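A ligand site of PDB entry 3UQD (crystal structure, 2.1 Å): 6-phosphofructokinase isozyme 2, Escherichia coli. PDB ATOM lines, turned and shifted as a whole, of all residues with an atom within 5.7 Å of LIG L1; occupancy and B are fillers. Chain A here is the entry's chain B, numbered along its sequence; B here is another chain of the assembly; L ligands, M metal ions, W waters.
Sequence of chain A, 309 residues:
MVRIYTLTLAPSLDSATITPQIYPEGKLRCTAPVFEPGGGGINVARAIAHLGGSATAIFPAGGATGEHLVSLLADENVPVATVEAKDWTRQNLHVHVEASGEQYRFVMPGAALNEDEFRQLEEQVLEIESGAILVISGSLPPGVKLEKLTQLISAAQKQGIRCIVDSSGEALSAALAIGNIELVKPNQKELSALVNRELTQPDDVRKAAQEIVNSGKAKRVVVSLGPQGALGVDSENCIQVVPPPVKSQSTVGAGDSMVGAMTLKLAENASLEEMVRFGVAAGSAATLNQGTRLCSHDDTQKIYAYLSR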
ATOM      1  N   ASP A 166      28.937  26.494  35.207  1.00  0.00           N
ATOM      2  CA  ASP A 166      28.074  25.436  34.672  1.00  0.00           C
ATOM      3  C   ASP A 166      28.846  24.136  34.647  1.00  0.00           C
ATOM      4  O   ASP A 166      29.635  23.885  33.732  1.00  0.00           O
ATOM      5  CB  ASP A 166      27.542  25.780  33.275  1.00  0.00           C
ATOM      6  CG  ASP A 166      26.597  24.720  32.716  1.00  0.00           C
ATOM      7  OD1 ASP A 166      26.244  23.772  33.449  1.00  0.00           O
ATOM      8  OD2 ASP A 166      26.203  24.822  31.535  1.00  0.00           O
ATOM      9  N   LYS A 185      23.581  27.044  36.228  1.00  0.00           N
ATOM     10  CA  LYS A 185      22.515  26.428  35.462  1.00  0.00           C
ATOM     11  C   LYS A 185      22.550  24.900  35.559  1.00  0.00           C
ATOM     12  O   LYS A 185      22.964  24.213  34.627  1.00  0.00           O
ATOM     13  CB  LYS A 185      22.561  26.863  33.996  1.00  0.00           C
ATOM     14  CG  LYS A 185      21.428  26.317  33.136  1.00  0.00           C
ATOM     15  CD  LYS A 185      21.901  26.115  31.713  1.00  0.00           C
ATOM     16  CE  LYS A 185      21.700  24.695  31.221  1.00  0.00           C
ATOM     17  NZ  LYS A 185      22.334  23.667  32.100  1.00  0.00           N
ATOM     18  N   ASN A 187      20.886  21.237  35.454  1.00  0.00           N
ATOM     19  CA  ASN A 187      19.667  20.601  34.961  1.00  0.00           C
ATOM     20  C   ASN A 187      19.002  19.887  36.119  1.00  0.00           C
ATOM     21  O   ASN A 187      19.432  20.040  37.265  1.00  0.00           O
ATOM     22  CB  ASN A 187      19.946  19.655  33.770  1.00  0.00           C
ATOM     23  CG  ASN A 187      20.925  18.531  34.117  1.00  0.00           C
ATOM     24  OD1 ASN A 187      20.969  18.034  35.244  1.00  0.00           O
ATOM     25  ND2 ASN A 187      21.719  18.121  33.128  1.00  0.00           N
ATOM     26  N   GLU A 190      21.285  17.318  37.907  1.00  0.00           N
ATOM     27  CA  GLU A 190      22.369  18.073  38.549  1.00  0.00           C
ATOM     28  C   GLU A 190      21.890  18.768  39.828  1.00  0.00           C
ATOM     29  O   GLU A 190      22.603  18.796  40.831  1.00  0.00           O
ATOM     30  CB  GLU A 190      22.984  19.093  37.566  1.00  0.00           C
ATOM     31  CG  GLU A 190      23.813  18.446  36.451  1.00  0.00           C
ATOM     32  CD  GLU A 190      24.276  19.424  35.380  1.00  0.00           C
ATOM     33  OE1 GLU A 190      25.165  19.043  34.579  1.00  0.00           O
ATOM     34  OE2 GLU A 190      23.766  20.557  35.313  1.00  0.00           O
ATOM     35  N   SER A 224      17.569  24.250  34.128  1.00  0.00           N
ATOM     36  CA  SER A 224      17.140  23.986  32.768  1.00  0.00           C
ATOM     37  C   SER A 224      16.360  22.682  32.708  1.00  0.00           C
ATOM     38  O   SER A 224      16.712  21.704  33.382  1.00  0.00           O
ATOM     39  CB  SER A 224      18.327  23.990  31.784  1.00  0.00           C
ATOM     40  OG  SER A 224      19.214  22.900  31.983  1.00  0.00           O
ATOM     41  N   LEU A 225      15.299  22.662  31.917  1.00  0.00           N
ATOM     42  CA  LEU A 225      14.336  21.584  31.990  1.00  0.00           C
ATOM     43  C   LEU A 225      14.128  20.906  30.645  1.00  0.00           C
ATOM     44  O   LEU A 225      13.054  20.353  30.378  1.00  0.00           O
ATOM     45  CB  LEU A 225      12.996  22.112  32.525  1.00  0.00           C
ATOM     46  CG  LEU A 225      13.006  22.867  33.862  1.00  0.00           C
ATOM     47  CD1 LEU A 225      11.627  23.454  34.155  1.00  0.00           C
ATOM     48  CD2 LEU A 225      13.445  21.950  35.005  1.00  0.00           C
ATOM     49  N   GLY A 226      15.152  20.962  29.797  1.00  0.00           N
ATOM     50  CA  GLY A 226      15.045  20.412  28.465  1.00  0.00           C
ATOM     51  C   GLY A 226      13.873  21.020  27.717  1.00  0.00           C
ATOM     52  O   GLY A 226      13.764  22.231  27.629  1.00  0.00           O
ATOM     53  N   PRO A 227      12.967  20.165  27.207  1.00  0.00           N
ATOM     54  CA  PRO A 227      11.783  20.594  26.445  1.00  0.00           C
ATOM     55  C   PRO A 227      10.865  21.538  27.246  1.00  0.00           C
ATOM     56  O   PRO A 227      10.131  22.329  26.650  1.00  0.00           O
ATOM     57  CB  PRO A 227      11.036  19.288  26.165  1.00  0.00           C
ATOM     58  CG  PRO A 227      12.040  18.216  26.375  1.00  0.00           C
ATOM     59  CD  PRO A 227      12.999  18.708  27.402  1.00  0.00           C
ATOM     60  N   GLY A 229      11.773  23.942  29.073  1.00  0.00           N
ATOM     61  CA  GLY A 229      12.371  25.254  29.211  1.00  0.00           C
ATOM     62  C   GLY A 229      13.231  25.381  30.441  1.00  0.00           C
ATOM     63  O   GLY A 229      14.128  24.568  30.653  1.00  0.00           O
ATOM     64  N   ALA A 230      12.962  26.386  31.261  1.00  0.00           N
ATOM     65  CA  ALA A 230      13.819  26.662  32.420  1.00  0.00           C
ATOM     66  C   ALA A 230      13.058  27.346  33.541  1.00  0.00           C
ATOM     67  O   ALA A 230      12.117  28.094  33.297  1.00  0.00           O
ATOM     68  CB  ALA A 230      15.011  27.511  31.998  1.00  0.00           C
ATOM     69  N   PRO A 243       9.445  26.806  26.019  1.00  0.00           N
ATOM     70  CA  PRO A 243       9.694  27.154  24.625  1.00  0.00           C
ATOM     71  C   PRO A 243       8.479  26.873  23.742  1.00  0.00           C
ATOM     72  O   PRO A 243       7.589  26.123  24.145  1.00  0.00           O
ATOM     73  CB  PRO A 243      10.850  26.233  24.233  1.00  0.00           C
ATOM     74  CG  PRO A 243      11.344  25.637  25.514  1.00  0.00           C
ATOM     75  CD  PRO A 243      10.181  25.602  26.414  1.00  0.00           C
ATOM     76  N   PRO A 244       8.450  27.460  22.532  1.00  0.00           N
ATOM     77  CA  PRO A 244       7.408  27.184  21.537  1.00  0.00           C
ATOM     78  C   PRO A 244       7.456  25.722  21.120  1.00  0.00           C
ATOM     79  O   PRO A 244       8.509  25.104  21.233  1.00  0.00           O
ATOM     80  CB  PRO A 244       7.823  28.049  20.339  1.00  0.00           C
ATOM     81  CG  PRO A 244       8.703  29.104  20.908  1.00  0.00           C
ATOM     82  CD  PRO A 244       9.420  28.455  22.037  1.00  0.00           C
ATOM     83  N   VAL A 246       8.302  23.729  18.768  1.00  0.00           N
ATOM     84  CA  VAL A 246       9.055  23.548  17.525  1.00  0.00           C
ATOM     85  C   VAL A 246       9.886  22.270  17.586  1.00  0.00           C
ATOM     86  O   VAL A 246      10.337  21.871  18.655  1.00  0.00           O
ATOM     87  CB  VAL A 246       9.955  24.756  17.203  1.00  0.00           C
ATOM     88  CG1 VAL A 246       9.103  26.004  16.958  1.00  0.00           C
ATOM     89  CG2 VAL A 246      10.957  24.999  18.317  1.00  0.00           C
ATOM     90  N   SER A 248      12.682  19.746  17.721  1.00  0.00           N
ATOM     91  CA  SER A 248      14.061  19.753  18.163  1.00  0.00           C
ATOM     92  C   SER A 248      14.854  18.678  17.431  1.00  0.00           C
ATOM     93  O   SER A 248      14.333  17.608  17.129  1.00  0.00           O
ATOM     94  CB  SER A 248      14.114  19.521  19.675  1.00  0.00           C
ATOM     95  OG  SER A 248      15.445  19.334  20.113  1.00  0.00           O
ATOM     96  N   THR A 251      20.773  18.494  20.413  1.00  0.00           N
ATOM     97  CA  THR A 251      20.710  19.263  21.647  1.00  0.00           C
ATOM     98  C   THR A 251      22.106  19.674  22.100  1.00  0.00           C
ATOM     99  O   THR A 251      22.275  20.352  23.115  1.00  0.00           O
ATOM    100  CB  THR A 251      20.002  18.453  22.763  1.00  0.00           C
ATOM    101  OG1 THR A 251      18.804  17.853  22.240  1.00  0.00           O
ATOM    102  CG2 THR A 251      19.633  19.335  23.943  1.00  0.00           C
ATOM    103  N   ALA A 254      23.012  23.141  23.599  1.00  0.00           N
ATOM    104  CA  ALA A 254      21.784  23.864  23.935  1.00  0.00           C
ATOM    105  C   ALA A 254      21.939  24.573  25.282  1.00  0.00           C
ATOM    106  O   ALA A 254      21.674  25.763  25.395  1.00  0.00           O
ATOM    107  CB  ALA A 254      20.599  22.907  23.970  1.00  0.00           C
ATOM    108  N   GLY A 255      22.393  23.830  26.275  1.00  0.00           N
ATOM    109  CA  GLY A 255      22.683  24.391  27.587  1.00  0.00           C
ATOM    110  C   GLY A 255      23.701  25.518  27.536  1.00  0.00           C
ATOM    111  O   GLY A 255      23.548  26.533  28.196  1.00  0.00           O
ATOM    112  N   MET A 258      22.183  28.642  25.992  1.00  0.00           N
ATOM    113  CA  MET A 258      21.373  29.245  27.051  1.00  0.00           C
ATOM    114  C   MET A 258      22.243  30.056  28.002  1.00  0.00           C
ATOM    115  O   MET A 258      21.950  31.223  28.261  1.00  0.00           O
ATOM    116  CB  MET A 258      20.612  28.154  27.817  1.00  0.00           C
ATOM    117  CG  MET A 258      20.041  28.630  29.163  1.00  0.00           C
ATOM    118  SD  MET A 258      18.947  27.428  29.966  1.00  0.00           S
ATOM    119  CE  MET A 258      17.423  27.771  29.107  1.00  0.00           C
ATOM    120  N   GLY A 279      17.492  33.128  27.522  1.00  0.00           N
ATOM    121  CA  GLY A 279      18.158  31.846  27.672  1.00  0.00           C
ATOM    122  C   GLY A 279      17.400  30.696  27.051  1.00  0.00           C
ATOM    123  O   GLY A 279      17.990  29.839  26.383  1.00  0.00           O
ATOM    124  N   VAL A 280      16.088  30.677  27.258  1.00  0.00           N
ATOM    125  CA  VAL A 280      15.239  29.650  26.672  1.00  0.00           C
ATOM    126  C   VAL A 280      15.184  29.831  25.157  1.00  0.00           C
ATOM    127  O   VAL A 280      15.205  28.849  24.412  1.00  0.00           O
ATOM    128  CB  VAL A 280      13.803  29.687  27.266  1.00  0.00           C
ATOM    129  CG1 VAL A 280      12.851  28.813  26.461  1.00  0.00           C
ATOM    130  CG2 VAL A 280      13.819  29.267  28.731  1.00  0.00           C
ATOM    131  N   ALA A 281      15.137  31.081  24.717  1.00  0.00           N
ATOM    132  CA  ALA A 281      15.156  31.371  23.283  1.00  0.00           C
ATOM    133  C   ALA A 281      16.427  30.834  22.630  1.00  0.00           C
ATOM    134  O   ALA A 281      16.371  30.158  21.598  1.00  0.00           O
ATOM    135  CB  ALA A 281      14.996  32.858  23.031  1.00  0.00           C
ATOM    136  N   GLY A 283      18.695  28.592  23.915  1.00  0.00           N
ATOM    137  CA  GLY A 283      18.768  27.157  24.104  1.00  0.00           C
ATOM    138  C   GLY A 283      17.894  26.400  23.114  1.00  0.00           C
ATOM    139  O   GLY A 283      18.331  25.406  22.527  1.00  0.00           O
ATOM    140  N   SER A 284      16.664  26.872  22.927  1.00  0.00           N
ATOM    141  CA  SER A 284      15.754  26.259  21.972  1.00  0.00           C
ATOM    142  C   SER A 284      16.171  26.522  20.526  1.00  0.00           C
ATOM    143  O   SER A 284      16.010  25.651  19.658  1.00  0.00           O
ATOM    144  CB  SER A 284      14.319  26.734  22.218  1.00  0.00           C
ATOM    145  OG  SER A 284      13.916  26.453  23.546  1.00  0.00           O
ATOM    146  N   THR A 287      18.641  24.007  19.215  1.00  0.00           N
ATOM    147  CA  THR A 287      18.199  22.634  18.999  1.00  0.00           C
ATOM    148  C   THR A 287      17.571  22.413  17.629  1.00  0.00           C
ATOM    149  O   THR A 287      17.180  21.287  17.297  1.00  0.00           O
ATOM    150  CB  THR A 287      17.183  22.152  20.059  1.00  0.00           C
ATOM    151  OG1 THR A 287      15.907  22.761  19.815  1.00  0.00           O
ATOM    152  CG2 THR A 287      17.650  22.487  21.468  1.00  0.00           C
ATOM    153  N   GLN B 228       5.684  19.278  27.054  1.00  0.00           N
ATOM    154  CA  GLN B 228       5.383  20.704  27.100  1.00  0.00           C
ATOM    155  C   GLN B 228       3.940  21.010  27.517  1.00  0.00           C
ATOM    156  O   GLN B 228       3.552  22.166  27.589  1.00  0.00           O
ATOM    157  CB  GLN B 228       5.728  21.365  25.758  1.00  0.00           C
ATOM    158  CG  GLN B 228       7.211  21.256  25.425  1.00  0.00           C
ATOM    159  CD  GLN B 228       7.589  21.976  24.146  1.00  0.00           C
ATOM    160  OE1 GLN B 228       6.797  22.063  23.205  1.00  0.00           O
ATOM    161  NE2 GLN B 228       8.810  22.498  24.110  1.00  0.00           N
HETATM  162  P1  LIG L   1      21.498  20.313  29.672  1.00  0.00           P
HETATM  163  O1  LIG L   1      20.653  19.281  30.367  1.00  0.00           O
HETATM  164  O2  LIG L   1      22.393  21.120  30.575  1.00  0.00           O
HETATM  165  O3  LIG L   1      22.176  19.746  28.448  1.00  0.00           O
HETATM  166  P2  LIG L   1      18.922  21.122  28.835  1.00  0.00           P
HETATM  167  O4  LIG L   1      18.186  21.504  30.100  1.00  0.00           O
HETATM  168  O5  LIG L   1      18.729  19.727  28.286  1.00  0.00           O
HETATM  169  O6  LIG L   1      20.487  21.393  29.069  1.00  0.00           O
HETATM  170  O7  LIG L   1      18.597  22.220  27.699  1.00  0.00           O
HETATM  171  C1  LIG L   1      18.889  23.591  27.930  1.00  0.00           C
HETATM  172  C2  LIG L   1      17.910  24.442  27.152  1.00  0.00           C
HETATM  173  O8  LIG L   1      17.880  24.036  25.780  1.00  0.00           O
HETATM  174  C3  LIG L   1      16.493  24.210  27.657  1.00  0.00           C
HETATM  175  O9  LIG L   1      16.160  25.024  28.770  1.00  0.00           O
HETATM  176  C4  LIG L   1      15.665  24.556  26.434  1.00  0.00           C
HETATM  177  O10 LIG L   1      15.548  25.976  26.337  1.00  0.00           O
HETATM  178  C5  LIG L   1      16.537  24.070  25.293  1.00  0.00           C
HETATM  179  N1  LIG L   1      16.107  22.698  24.946  1.00  0.00           N
HETATM  180  C6  LIG L   1      16.782  21.570  25.254  1.00  0.00           C
HETATM  181  N2  LIG L   1      16.122  20.478  24.779  1.00  0.00           N
HETATM  182  C7  LIG L   1      15.000  20.915  24.172  1.00  0.00           C
HETATM  183  C8  LIG L   1      13.859  20.287  23.460  1.00  0.00           C
HETATM  184  N3  LIG L   1      13.787  18.949  23.311  1.00  0.00           N
HETATM  185  N4  LIG L   1      12.905  21.099  22.963  1.00  0.00           N
HETATM  186  C9  LIG L   1      12.960  22.432  23.113  1.00  0.00           C
HETATM  187  N5  LIG L   1      13.966  23.069  23.747  1.00  0.00           N
HETATM  188  C10 LIG L   1      14.992  22.373  24.290  1.00  0.00           C
HETATM  189  P1  LG2 L   2      26.214  19.553  26.000  1.00  0.00           P
HETATM  190  O1  LG2 L   2      26.306  19.472  27.572  1.00  0.00           O
HETATM  191  O2  LG2 L   2      25.984  18.216  25.360  1.00  0.00           O
HETATM  192  O3  LG2 L   2      25.115  20.509  25.626  1.00  0.00           O
HETATM  193  O4  LG2 L   2      27.591  20.248  25.627  1.00  0.00           O
HETATM  194  C1  LG2 L   2      28.241  20.030  24.391  1.00  0.00           C
HETATM  195  C2  LG2 L   2      29.702  19.716  24.494  1.00  0.00           C
HETATM  196  O5  LG2 L   2      30.350  20.814  25.079  1.00  0.00           O
HETATM  197  C3  LG2 L   2      30.305  19.310  23.233  1.00  0.00           C
HETATM  198  O6  LG2 L   2      30.699  20.423  22.518  1.00  0.00           O
HETATM  199  C4  LG2 L   2      31.430  18.534  23.685  1.00  0.00           C
HETATM  200  O7  LG2 L   2      31.737  17.587  22.698  1.00  0.00           O
HETATM  201  C5  LG2 L   2      30.946  17.880  24.876  1.00  0.00           C
HETATM  202  O8  LG2 L   2      29.834  18.639  25.346  1.00  0.00           O
HETATM  203  C6  LG2 L   2      31.929  17.835  25.977  1.00  0.00           C
HETATM  204  O9  LG2 L   2      31.433  17.297  27.177  1.00  0.00           O
HETATM  205  P2  LG2 L   2      32.223  17.368  28.536  1.00  0.00           P
HETATM  206  O10 LG2 L   2      31.219  17.007  29.701  1.00  0.00           O
HETATM  207  O11 LG2 L   2      32.661  18.806  28.734  1.00  0.00           O
HETATM  208  O12 LG2 L   2      33.401  16.410  28.532  1.00  0.00           O
HETATM  209 MG    MG M   1      25.140  20.616  30.958  1.00  0.00          MG
HETATM  210  O   HOH W   1      22.761  20.924  26.174  1.00  0.00           O
HETATM  211  O   HOH W   2      20.780  17.851  27.347  1.00  0.00           O
HETATM  212  O   HOH W   3      10.599  20.656  21.500  1.00  0.00           O
HETATM  213  O   HOH W   4      16.825  16.950  28.697  1.00  0.00           O
HETATM  214  O   HOH W   5      24.490  22.092  33.202  1.00  0.00           O
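OG of Ser 224 is in hydrogen-bond range of O4 of LIG L1, at 2.6 Å. O of Gly 229 is in hydrogen-bond range of O9 of LIG L1, 2.8 Å away. NZ of Lys 185 lies within salt-bridge range of O2 of LIG L1. N of Gly 226 is in hydrogen-bond range of O4 of LIG L1, at 3.1 Å. O1 of LIG L1 lies within hydrogen-bond range of ND2 of Asn 187 (3.2 Å). The side-chain hydroxyl (OG) of Ser 284 is in hydrogen-bond range of an oxygen (O10) of LIG L1 (3.3 Å). The backbone carbonyl oxygen of Val 280 is in hydrogen-bond range of an oxygen (O10) of LIG L1, 3.5 Å away.
OG of Ser 224 sits close to NZ of Lys 185. The side-chain amide oxygen (OD1) of Asn 187 is in hydrogen-bond range of the backbone NH (N) of Glu 190, at 2.8 Å. The backbone carbonyl oxygen of Val 280 is in hydrogen-bond range of the side-chain hydroxyl of Ser 284. The backbone carbonyl oxygen of Ser 284 sits at hydrogen-bond distance from the side-chain hydroxyl of Thr 287 (2.9 Å). NE2 of Gln 228 of chain B sits at hydrogen-bond distance from O of Pro 227, at 2.9 Å. The side-chain hydroxyl of Ser 248 lies close to the side-chain hydroxyl of Thr 287 (3.5 Å).
Merely in contact with LIG L1: Met 258, Ala 254, Gly 283, Leu 225, Pro 227, Ser 248, Thr 251, Thr 287 and Gly 255. Of the 25 residues printed, 16 come within 4 Å of LIG L1. The nearest printed residue that does not touch LIG L1 is Pro 243 (4.1 Å).
Water W1 lies within hydrogen-bond range of O3 of LG2 L2 (2.5 Å), O3 of LIG L1 (2.6 Å), N of Gly 255 (2.9 Å), O of Thr 251 (3.1 Å) and N of Ala 254 (3.4 Å). Water W3 lies within hydrogen-bond range of N4 of LIG L1 (2.8 Å) and O of Val 246 (3.1 Å). Water W5 lies within hydrogen-bond range of OD1 of Asp 166 (2.4 Å), OE2 of Glu 190 (2.7 Å), NZ of Lys 185 (2.9 Å) and O2 of LIG L1 (3.5 Å).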
